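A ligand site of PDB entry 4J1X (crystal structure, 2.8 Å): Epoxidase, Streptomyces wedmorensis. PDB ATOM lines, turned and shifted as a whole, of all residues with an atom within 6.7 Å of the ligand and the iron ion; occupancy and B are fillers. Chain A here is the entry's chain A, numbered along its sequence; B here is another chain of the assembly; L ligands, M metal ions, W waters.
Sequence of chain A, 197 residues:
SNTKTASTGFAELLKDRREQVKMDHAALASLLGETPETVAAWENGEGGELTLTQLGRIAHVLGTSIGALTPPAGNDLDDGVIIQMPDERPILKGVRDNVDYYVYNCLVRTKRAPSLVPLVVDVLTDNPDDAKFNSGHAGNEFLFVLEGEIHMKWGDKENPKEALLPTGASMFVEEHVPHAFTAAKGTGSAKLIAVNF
Water W2 lies within hydrogen-bond range of OD1 of Asn 196 (2.7 Å) and O4 of the ligand (3.4 Å). Water W1 lies within hydrogen-bond range of NH1 of Arg 96 (2.9 Å), O of His 179 (3.0 Å), ND2 of Asn 134 (3.0 Å), O1 of the ligand (3.0 Å) and OH of Tyr 102 (3.1 Å).
Asn 134 touches the iron ion (ND2 to FE, 3.96 Å). Of the 22 residues printed, 4 come within 4 Å of the iron ion. The nearest printed residue that does not touch the iron ion is Asn 196 (4.4 Å).
An oxygen (O1) of the ligand lies within salt-bridge range of the guanidinium group of Arg 96, 2.5 Å away. An oxygen (O2) of the ligand lies close to the side-chain amide nitrogen of Asn 134 (2.7 Å). NZ of Lys 22 of chain B lies within salt-bridge range of O4 of the ligand (2.8 Å). O4 of the ligand sits at hydrogen-bond distance from OH of Tyr 104, 3.3 Å away.
Residues that only touch the ligand: Tyr 102 (3.3 Å), Phe 181 (3.5 Å) and Leu 192 (3.9 Å). Hydrophobic or aromatic side chains that line the ligand: Tyr 102, Tyr 104, His 137, His 179, Phe 181 and Leu 192. Ten residues have an atom within 4 Å of the ligand: Arg 96, Tyr 102, Tyr 104, Asn 134, His 137, Glu 141, His 179, Phe 181, Leu 192 and Lys 22 of chain B.
OE1 of Glu 141 lies close to OD1 of Asn 196. The backbone carbonyl oxygen (O) of Glu 141 lies within hydrogen-bond range of the backbone NH (N) of Val 173 (3.0 Å). The side-chain amide oxygen of Asn 134 lies within hydrogen-bond range of the backbone NH of His 179. A ring nitrogen (ND1) of His 179 is in hydrogen-bond range of the backbone carbonyl oxygen of Val 177 (2.7 Å). The backbone carbonyl oxygen of Lys 132 is in hydrogen-bond range of the guanidinium group of Arg 96, at 2.6 Å. The backbone NH of Gly 136 is in hydrogen-bond range of the side-chain amide oxygen of Asn 134, at 2.9 Å. The backbone NH of Phe 181 lies within hydrogen-bond range of the side-chain hydroxyl of Tyr 102, 3.0 Å away. N of Val 121 lies within hydrogen-bond range of O of Leu 192, 2.7 Å away.
The iron ion is bound by an oxygen (O2) of the ligand (2.0 Å), a ring nitrogen (NE2) of His 137 (2.1 Å), the side-chain carboxylate (OE1) of Glu 141 (2.2 Å), a ring nitrogen (NE2) of His 179 (2.2 Å) and an oxygen (O3) of the ligand (2.3 Å).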
ATOM      1  N   ARG A  96       7.364  12.335  -7.189  1.00  0.00           N
ATOM      2  CA  ARG A  96       7.621  13.661  -7.736  1.00  0.00           C
ATOM      3  C   ARG A  96       7.226  14.691  -6.682  1.00  0.00           C
ATOM      4  O   ARG A  96       6.047  14.812  -6.329  1.00  0.00           O
ATOM      5  CB  ARG A  96       6.819  13.891  -9.020  1.00  0.00           C
ATOM      6  CG  ARG A  96       7.259  13.006 -10.156  1.00  0.00           C
ATOM      7  CD  ARG A  96       6.526  13.304 -11.446  1.00  0.00           C
ATOM      8  NE  ARG A  96       6.918  12.349 -12.481  1.00  0.00           N
ATOM      9  CZ  ARG A  96       6.424  12.329 -13.713  1.00  0.00           C
ATOM     10  NH1 ARG A  96       5.512  13.215 -14.101  1.00  0.00           N
ATOM     11  NH2 ARG A  96       6.856  11.404 -14.564  1.00  0.00           N
ATOM     12  N   TYR A 102       2.927   8.339  -9.243  1.00  0.00           N
ATOM     13  CA  TYR A 102       2.629   7.180 -10.063  1.00  0.00           C
ATOM     14  C   TYR A 102       3.043   5.885  -9.381  1.00  0.00           C
ATOM     15  O   TYR A 102       3.712   5.885  -8.345  1.00  0.00           O
ATOM     16  CB  TYR A 102       3.386   7.262 -11.396  1.00  0.00           C
ATOM     17  CG  TYR A 102       3.019   8.394 -12.357  1.00  0.00           C
ATOM     18  CD1 TYR A 102       3.989   8.905 -13.232  1.00  0.00           C
ATOM     19  CD2 TYR A 102       1.719   8.890 -12.448  1.00  0.00           C
ATOM     20  CE1 TYR A 102       3.672   9.882 -14.172  1.00  0.00           C
ATOM     21  CE2 TYR A 102       1.386   9.881 -13.389  1.00  0.00           C
ATOM     22  CZ  TYR A 102       2.380  10.361 -14.257  1.00  0.00           C
ATOM     23  OH  TYR A 102       2.083  11.332 -15.206  1.00  0.00           O
ATOM     24  N   TYR A 104       4.473   2.291 -11.088  1.00  0.00           N
ATOM     25  CA  TYR A 104       4.787   1.588 -12.324  1.00  0.00           C
ATOM     26  C   TYR A 104       4.786   0.075 -12.243  1.00  0.00           C
ATOM     27  O   TYR A 104       5.587  -0.525 -11.540  1.00  0.00           O
ATOM     28  CB  TYR A 104       6.146   2.030 -12.860  1.00  0.00           C
ATOM     29  CG  TYR A 104       6.256   3.489 -13.170  1.00  0.00           C
ATOM     30  CD1 TYR A 104       6.684   4.391 -12.202  1.00  0.00           C
ATOM     31  CD2 TYR A 104       5.976   3.967 -14.455  1.00  0.00           C
ATOM     32  CE1 TYR A 104       6.848   5.736 -12.507  1.00  0.00           C
ATOM     33  CE2 TYR A 104       6.149   5.315 -14.766  1.00  0.00           C
ATOM     34  CZ  TYR A 104       6.589   6.191 -13.789  1.00  0.00           C
ATOM     35  OH  TYR A 104       6.802   7.510 -14.105  1.00  0.00           O
ATOM     36  N   LEU A 119       4.144  -0.477 -19.752  1.00  0.00           N
ATOM     37  CA  LEU A 119       3.786  -0.324 -18.352  1.00  0.00           C
ATOM     38  C   LEU A 119       2.300  -0.169 -18.097  1.00  0.00           C
ATOM     39  O   LEU A 119       1.558   0.332 -18.956  1.00  0.00           O
ATOM     40  CB  LEU A 119       4.452   0.946 -17.821  1.00  0.00           C
ATOM     41  CG  LEU A 119       5.953   1.145 -17.998  1.00  0.00           C
ATOM     42  CD1 LEU A 119       6.256   2.645 -17.980  1.00  0.00           C
ATOM     43  CD2 LEU A 119       6.696   0.398 -16.885  1.00  0.00           C
ATOM     44  N   VAL A 121       0.245   1.868 -15.625  1.00  0.00           N
ATOM     45  CA  VAL A 121       0.504   2.949 -14.677  1.00  0.00           C
ATOM     46  C   VAL A 121      -0.689   3.348 -13.808  1.00  0.00           C
ATOM     47  O   VAL A 121      -1.803   3.577 -14.297  1.00  0.00           O
ATOM     48  CB  VAL A 121       1.016   4.214 -15.411  1.00  0.00           C
ATOM     49  CG1 VAL A 121       1.351   5.301 -14.392  1.00  0.00           C
ATOM     50  CG2 VAL A 121       2.242   3.865 -16.253  1.00  0.00           C
ATOM     51  N   VAL A 123      -2.222   6.117 -11.842  1.00  0.00           N
ATOM     52  CA  VAL A 123      -2.203   7.570 -11.694  1.00  0.00           C
ATOM     53  C   VAL A 123      -2.866   7.827 -10.333  1.00  0.00           C
ATOM     54  O   VAL A 123      -4.102   7.748 -10.189  1.00  0.00           O
ATOM     55  CB  VAL A 123      -3.025   8.225 -12.822  1.00  0.00           C
ATOM     56  CG1 VAL A 123      -2.825   9.725 -12.824  1.00  0.00           C
ATOM     57  CG2 VAL A 123      -2.630   7.634 -14.153  1.00  0.00           C
ATOM     58  N   LYS A 132       2.444  17.192 -12.241  1.00  0.00           N
ATOM     59  CA  LYS A 132       3.884  17.349 -12.290  1.00  0.00           C
ATOM     60  C   LYS A 132       4.474  16.759 -13.561  1.00  0.00           C
ATOM     61  O   LYS A 132       4.323  15.566 -13.844  1.00  0.00           O
ATOM     62  CB  LYS A 132       4.514  16.707 -11.059  1.00  0.00           C
ATOM     63  CG  LYS A 132       3.806  17.157  -9.786  1.00  0.00           C
ATOM     64  CD  LYS A 132       4.583  16.859  -8.522  1.00  0.00           C
ATOM     65  CE  LYS A 132       3.861  17.442  -7.315  1.00  0.00           C
ATOM     66  NZ  LYS A 132       3.559  18.895  -7.501  1.00  0.00           N
ATOM     67  N   ASN A 134       7.452  15.872 -16.584  1.00  0.00           N
ATOM     68  CA  ASN A 134       8.740  15.244 -16.705  1.00  0.00           C
ATOM     69  C   ASN A 134       9.316  16.154 -17.787  1.00  0.00           C
ATOM     70  O   ASN A 134       8.572  16.936 -18.391  1.00  0.00           O
ATOM     71  CB  ASN A 134       8.630  13.798 -17.218  1.00  0.00           C
ATOM     72  CG  ASN A 134       7.725  13.664 -18.428  1.00  0.00           C
ATOM     73  OD1 ASN A 134       7.693  14.535 -19.304  1.00  0.00           O
ATOM     74  ND2 ASN A 134       6.994  12.570 -18.492  1.00  0.00           N
ATOM     75  N   GLY A 136      10.089  15.549 -20.674  1.00  0.00           N
ATOM     76  CA  GLY A 136       9.988  14.871 -21.953  1.00  0.00           C
ATOM     77  C   GLY A 136      11.069  13.788 -21.946  1.00  0.00           C
ATOM     78  O   GLY A 136      11.922  13.783 -21.039  1.00  0.00           O
ATOM     79  N   HIS A 137      11.067  12.884 -22.919  1.00  0.00           N
ATOM     80  CA  HIS A 137      12.082  11.826 -22.943  1.00  0.00           C
ATOM     81  C   HIS A 137      12.270  11.227 -24.335  1.00  0.00           C
ATOM     82  O   HIS A 137      11.447  11.427 -25.227  1.00  0.00           O
ATOM     83  CB  HIS A 137      11.727  10.726 -21.943  1.00  0.00           C
ATOM     84  CG  HIS A 137      10.334  10.205 -22.081  1.00  0.00           C
ATOM     85  ND1 HIS A 137       9.864   9.503 -23.183  1.00  0.00           N
ATOM     86  CD2 HIS A 137       9.275  10.307 -21.241  1.00  0.00           C
ATOM     87  CE1 HIS A 137       8.570   9.199 -22.963  1.00  0.00           C
ATOM     88  NE2 HIS A 137       8.165   9.675 -21.802  1.00  0.00           N
ATOM     89  N   GLU A 141       5.784   7.404 -27.296  1.00  0.00           N
ATOM     90  CA  GLU A 141       5.011   6.708 -26.295  1.00  0.00           C
ATOM     91  C   GLU A 141       3.562   6.578 -26.698  1.00  0.00           C
ATOM     92  O   GLU A 141       2.917   7.561 -27.053  1.00  0.00           O
ATOM     93  CB  GLU A 141       5.102   7.454 -24.975  1.00  0.00           C
ATOM     94  CG  GLU A 141       4.528   6.723 -23.799  1.00  0.00           C
ATOM     95  CD  GLU A 141       4.587   7.558 -22.547  1.00  0.00           C
ATOM     96  OE1 GLU A 141       5.495   8.429 -22.465  1.00  0.00           O
ATOM     97  OE2 GLU A 141       3.748   7.334 -21.645  1.00  0.00           O
ATOM     98  N   LEU A 143      -0.245   5.542 -25.492  1.00  0.00           N
ATOM     99  CA  LEU A 143      -1.014   5.431 -24.253  1.00  0.00           C
ATOM    100  C   LEU A 143      -2.456   5.024 -24.491  1.00  0.00           C
ATOM    101  O   LEU A 143      -3.072   5.379 -25.500  1.00  0.00           O
ATOM    102  CB  LEU A 143      -0.970   6.735 -23.462  1.00  0.00           C
ATOM    103  CG  LEU A 143       0.413   7.139 -22.961  1.00  0.00           C
ATOM    104  CD1 LEU A 143       0.770   8.486 -23.552  1.00  0.00           C
ATOM    105  CD2 LEU A 143       0.435   7.174 -21.438  1.00  0.00           C
ATOM    106  N   VAL A 173       2.388  10.443 -27.744  1.00  0.00           N
ATOM    107  CA  VAL A 173       3.180  11.595 -27.354  1.00  0.00           C
ATOM    108  C   VAL A 173       4.544  11.407 -28.009  1.00  0.00           C
ATOM    109  O   VAL A 173       5.219  10.412 -27.757  1.00  0.00           O
ATOM    110  CB  VAL A 173       3.366  11.669 -25.819  1.00  0.00           C
ATOM    111  CG1 VAL A 173       4.325  12.789 -25.451  1.00  0.00           C
ATOM    112  CG2 VAL A 173       2.027  11.897 -25.151  1.00  0.00           C
ATOM    113  N   VAL A 177       8.662  15.490 -26.054  1.00  0.00           N
ATOM    114  CA  VAL A 177       7.516  16.293 -25.651  1.00  0.00           C
ATOM    115  C   VAL A 177       7.231  16.054 -24.169  1.00  0.00           C
ATOM    116  O   VAL A 177       7.087  14.919 -23.735  1.00  0.00           O
ATOM    117  CB  VAL A 177       6.255  15.925 -26.473  1.00  0.00           C
ATOM    118  CG1 VAL A 177       5.070  16.748 -25.996  1.00  0.00           C
ATOM    119  CG2 VAL A 177       6.504  16.152 -27.940  1.00  0.00           C
ATOM    120  N   HIS A 179       5.173  15.838 -20.659  1.00  0.00           N
ATOM    121  CA  HIS A 179       3.798  15.495 -20.339  1.00  0.00           C
ATOM    122  C   HIS A 179       3.570  15.213 -18.861  1.00  0.00           C
ATOM    123  O   HIS A 179       4.507  15.045 -18.096  1.00  0.00           O
ATOM    124  CB  HIS A 179       3.335  14.289 -21.191  1.00  0.00           C
ATOM    125  CG  HIS A 179       4.381  13.222 -21.347  1.00  0.00           C
ATOM    126  ND1 HIS A 179       5.564  13.403 -22.034  1.00  0.00           N
ATOM    127  CD2 HIS A 179       4.402  11.949 -20.904  1.00  0.00           C
ATOM    128  CE1 HIS A 179       6.247  12.252 -21.991  1.00  0.00           C
ATOM    129  NE2 HIS A 179       5.585  11.336 -21.320  1.00  0.00           N
ATOM    130  N   ALA A 180       2.293  15.177 -18.481  1.00  0.00           N
ATOM    131  CA  ALA A 180       1.907  14.910 -17.095  1.00  0.00           C
ATOM    132  C   ALA A 180       0.487  14.385 -17.081  1.00  0.00           C
ATOM    133  O   ALA A 180      -0.327  14.748 -17.927  1.00  0.00           O
ATOM    134  CB  ALA A 180       1.992  16.194 -16.287  1.00  0.00           C
ATOM    135  N   PHE A 181       0.192  13.525 -16.115  1.00  0.00           N
ATOM    136  CA  PHE A 181      -1.134  12.934 -15.993  1.00  0.00           C
ATOM    137  C   PHE A 181      -1.609  12.944 -14.538  1.00  0.00           C
ATOM    138  O   PHE A 181      -0.809  12.942 -13.616  1.00  0.00           O
ATOM    139  CB  PHE A 181      -1.111  11.469 -16.450  1.00  0.00           C
ATOM    140  CG  PHE A 181      -0.750  11.278 -17.893  1.00  0.00           C
ATOM    141  CD1 PHE A 181      -1.648  11.612 -18.897  1.00  0.00           C
ATOM    142  CD2 PHE A 181       0.504  10.771 -18.247  1.00  0.00           C
ATOM    143  CE1 PHE A 181      -1.311  11.443 -20.247  1.00  0.00           C
ATOM    144  CE2 PHE A 181       0.849  10.598 -19.586  1.00  0.00           C
ATOM    145  CZ  PHE A 181      -0.065  10.934 -20.595  1.00  0.00           C
ATOM    146  N   LEU A 192      -3.687   3.808 -16.699  1.00  0.00           N
ATOM    147  CA  LEU A 192      -3.452   3.784 -18.125  1.00  0.00           C
ATOM    148  C   LEU A 192      -2.287   2.877 -18.483  1.00  0.00           C
ATOM    149  O   LEU A 192      -1.405   2.619 -17.666  1.00  0.00           O
ATOM    150  CB  LEU A 192      -3.227   5.213 -18.666  1.00  0.00           C
ATOM    151  CG  LEU A 192      -2.211   6.136 -17.989  1.00  0.00           C
ATOM    152  CD1 LEU A 192      -0.853   5.511 -18.099  1.00  0.00           C
ATOM    153  CD2 LEU A 192      -2.227   7.512 -18.635  1.00  0.00           C
ATOM    154  N   ALA A 194       0.952   2.380 -20.649  1.00  0.00           N
ATOM    155  CA  ALA A 194       1.899   3.228 -21.347  1.00  0.00           C
ATOM    156  C   ALA A 194       2.912   2.357 -22.040  1.00  0.00           C
ATOM    157  O   ALA A 194       3.527   1.494 -21.415  1.00  0.00           O
ATOM    158  CB  ALA A 194       2.593   4.155 -20.352  1.00  0.00           C
ATOM    159  N   ASN A 196       6.336   2.538 -24.243  1.00  0.00           N
ATOM    160  CA  ASN A 196       7.455   3.285 -24.841  1.00  0.00           C
ATOM    161  C   ASN A 196       8.108   2.369 -25.868  1.00  0.00           C
ATOM    162  O   ASN A 196       8.417   1.212 -25.562  1.00  0.00           O
ATOM    163  CB  ASN A 196       8.496   3.654 -23.785  1.00  0.00           C
ATOM    164  CG  ASN A 196       7.942   4.572 -22.724  1.00  0.00           C
ATOM    165  OD1 ASN A 196       7.680   5.762 -22.972  1.00  0.00           O
ATOM    166  ND2 ASN A 196       7.733   4.030 -21.525  1.00  0.00           N
ATOM    167  N   GLU B  19      16.413   4.715 -15.501  1.00  0.00           N
ATOM    168  CA  GLU B  19      15.149   5.440 -15.404  1.00  0.00           C
ATOM    169  C   GLU B  19      14.157   4.939 -16.469  1.00  0.00           C
ATOM    170  O   GLU B  19      12.966   4.794 -16.213  1.00  0.00           O
ATOM    171  CB  GLU B  19      15.399   6.936 -15.580  1.00  0.00           C
ATOM    172  CG  GLU B  19      16.282   7.510 -14.487  1.00  0.00           C
ATOM    173  CD  GLU B  19      16.522   9.029 -14.618  1.00  0.00           C
ATOM    174  OE1 GLU B  19      17.105   9.605 -13.659  1.00  0.00           O
ATOM    175  OE2 GLU B  19      16.145   9.635 -15.652  1.00  0.00           O
ATOM    176  N   LYS B  22      12.210   2.163 -15.341  1.00  0.00           N
ATOM    177  CA  LYS B  22      11.667   2.496 -14.034  1.00  0.00           C
ATOM    178  C   LYS B  22      12.307   1.764 -12.869  1.00  0.00           C
ATOM    179  O   LYS B  22      11.630   1.024 -12.147  1.00  0.00           O
ATOM    180  CB  LYS B  22      10.149   2.253 -14.016  1.00  0.00           C
ATOM    181  CG  LYS B  22       9.413   2.748 -15.248  1.00  0.00           C
ATOM    182  CD  LYS B  22       9.669   4.213 -15.512  1.00  0.00           C
ATOM    183  CE  LYS B  22       8.957   4.646 -16.782  1.00  0.00           C
ATOM    184  NZ  LYS B  22       9.492   5.937 -17.321  1.00  0.00           N
HETATM  185  C1  LIG L   1       4.806   8.115 -18.233  1.00  0.00           C
HETATM  186  C2  LIG L   1       3.588   8.455 -17.364  1.00  0.00           C
HETATM  187  C3  LIG L   1       2.314   7.755 -17.826  1.00  0.00           C
HETATM  188  O1  LIG L   1       6.126   9.865 -16.401  1.00  0.00           O
HETATM  189  O2  LIG L   1       6.929   9.854 -18.871  1.00  0.00           O
HETATM  190  P1  LIG L   1       6.390   8.949 -17.667  1.00  0.00           P
HETATM  191  O3  LIG L   1       4.553   8.536 -19.550  1.00  0.00           O
HETATM  192  O4  LIG L   1       7.478   7.838 -17.299  1.00  0.00           O
HETATM  193 FE    FE M   1       6.353   9.355 -20.711  1.00  0.00          FE
HETATM  194  O   HOH W   1       4.579  12.436 -16.721  1.00  0.00           O
HETATM  195  O   HOH W   2       7.005   6.448 -20.409  1.00  0.00           O
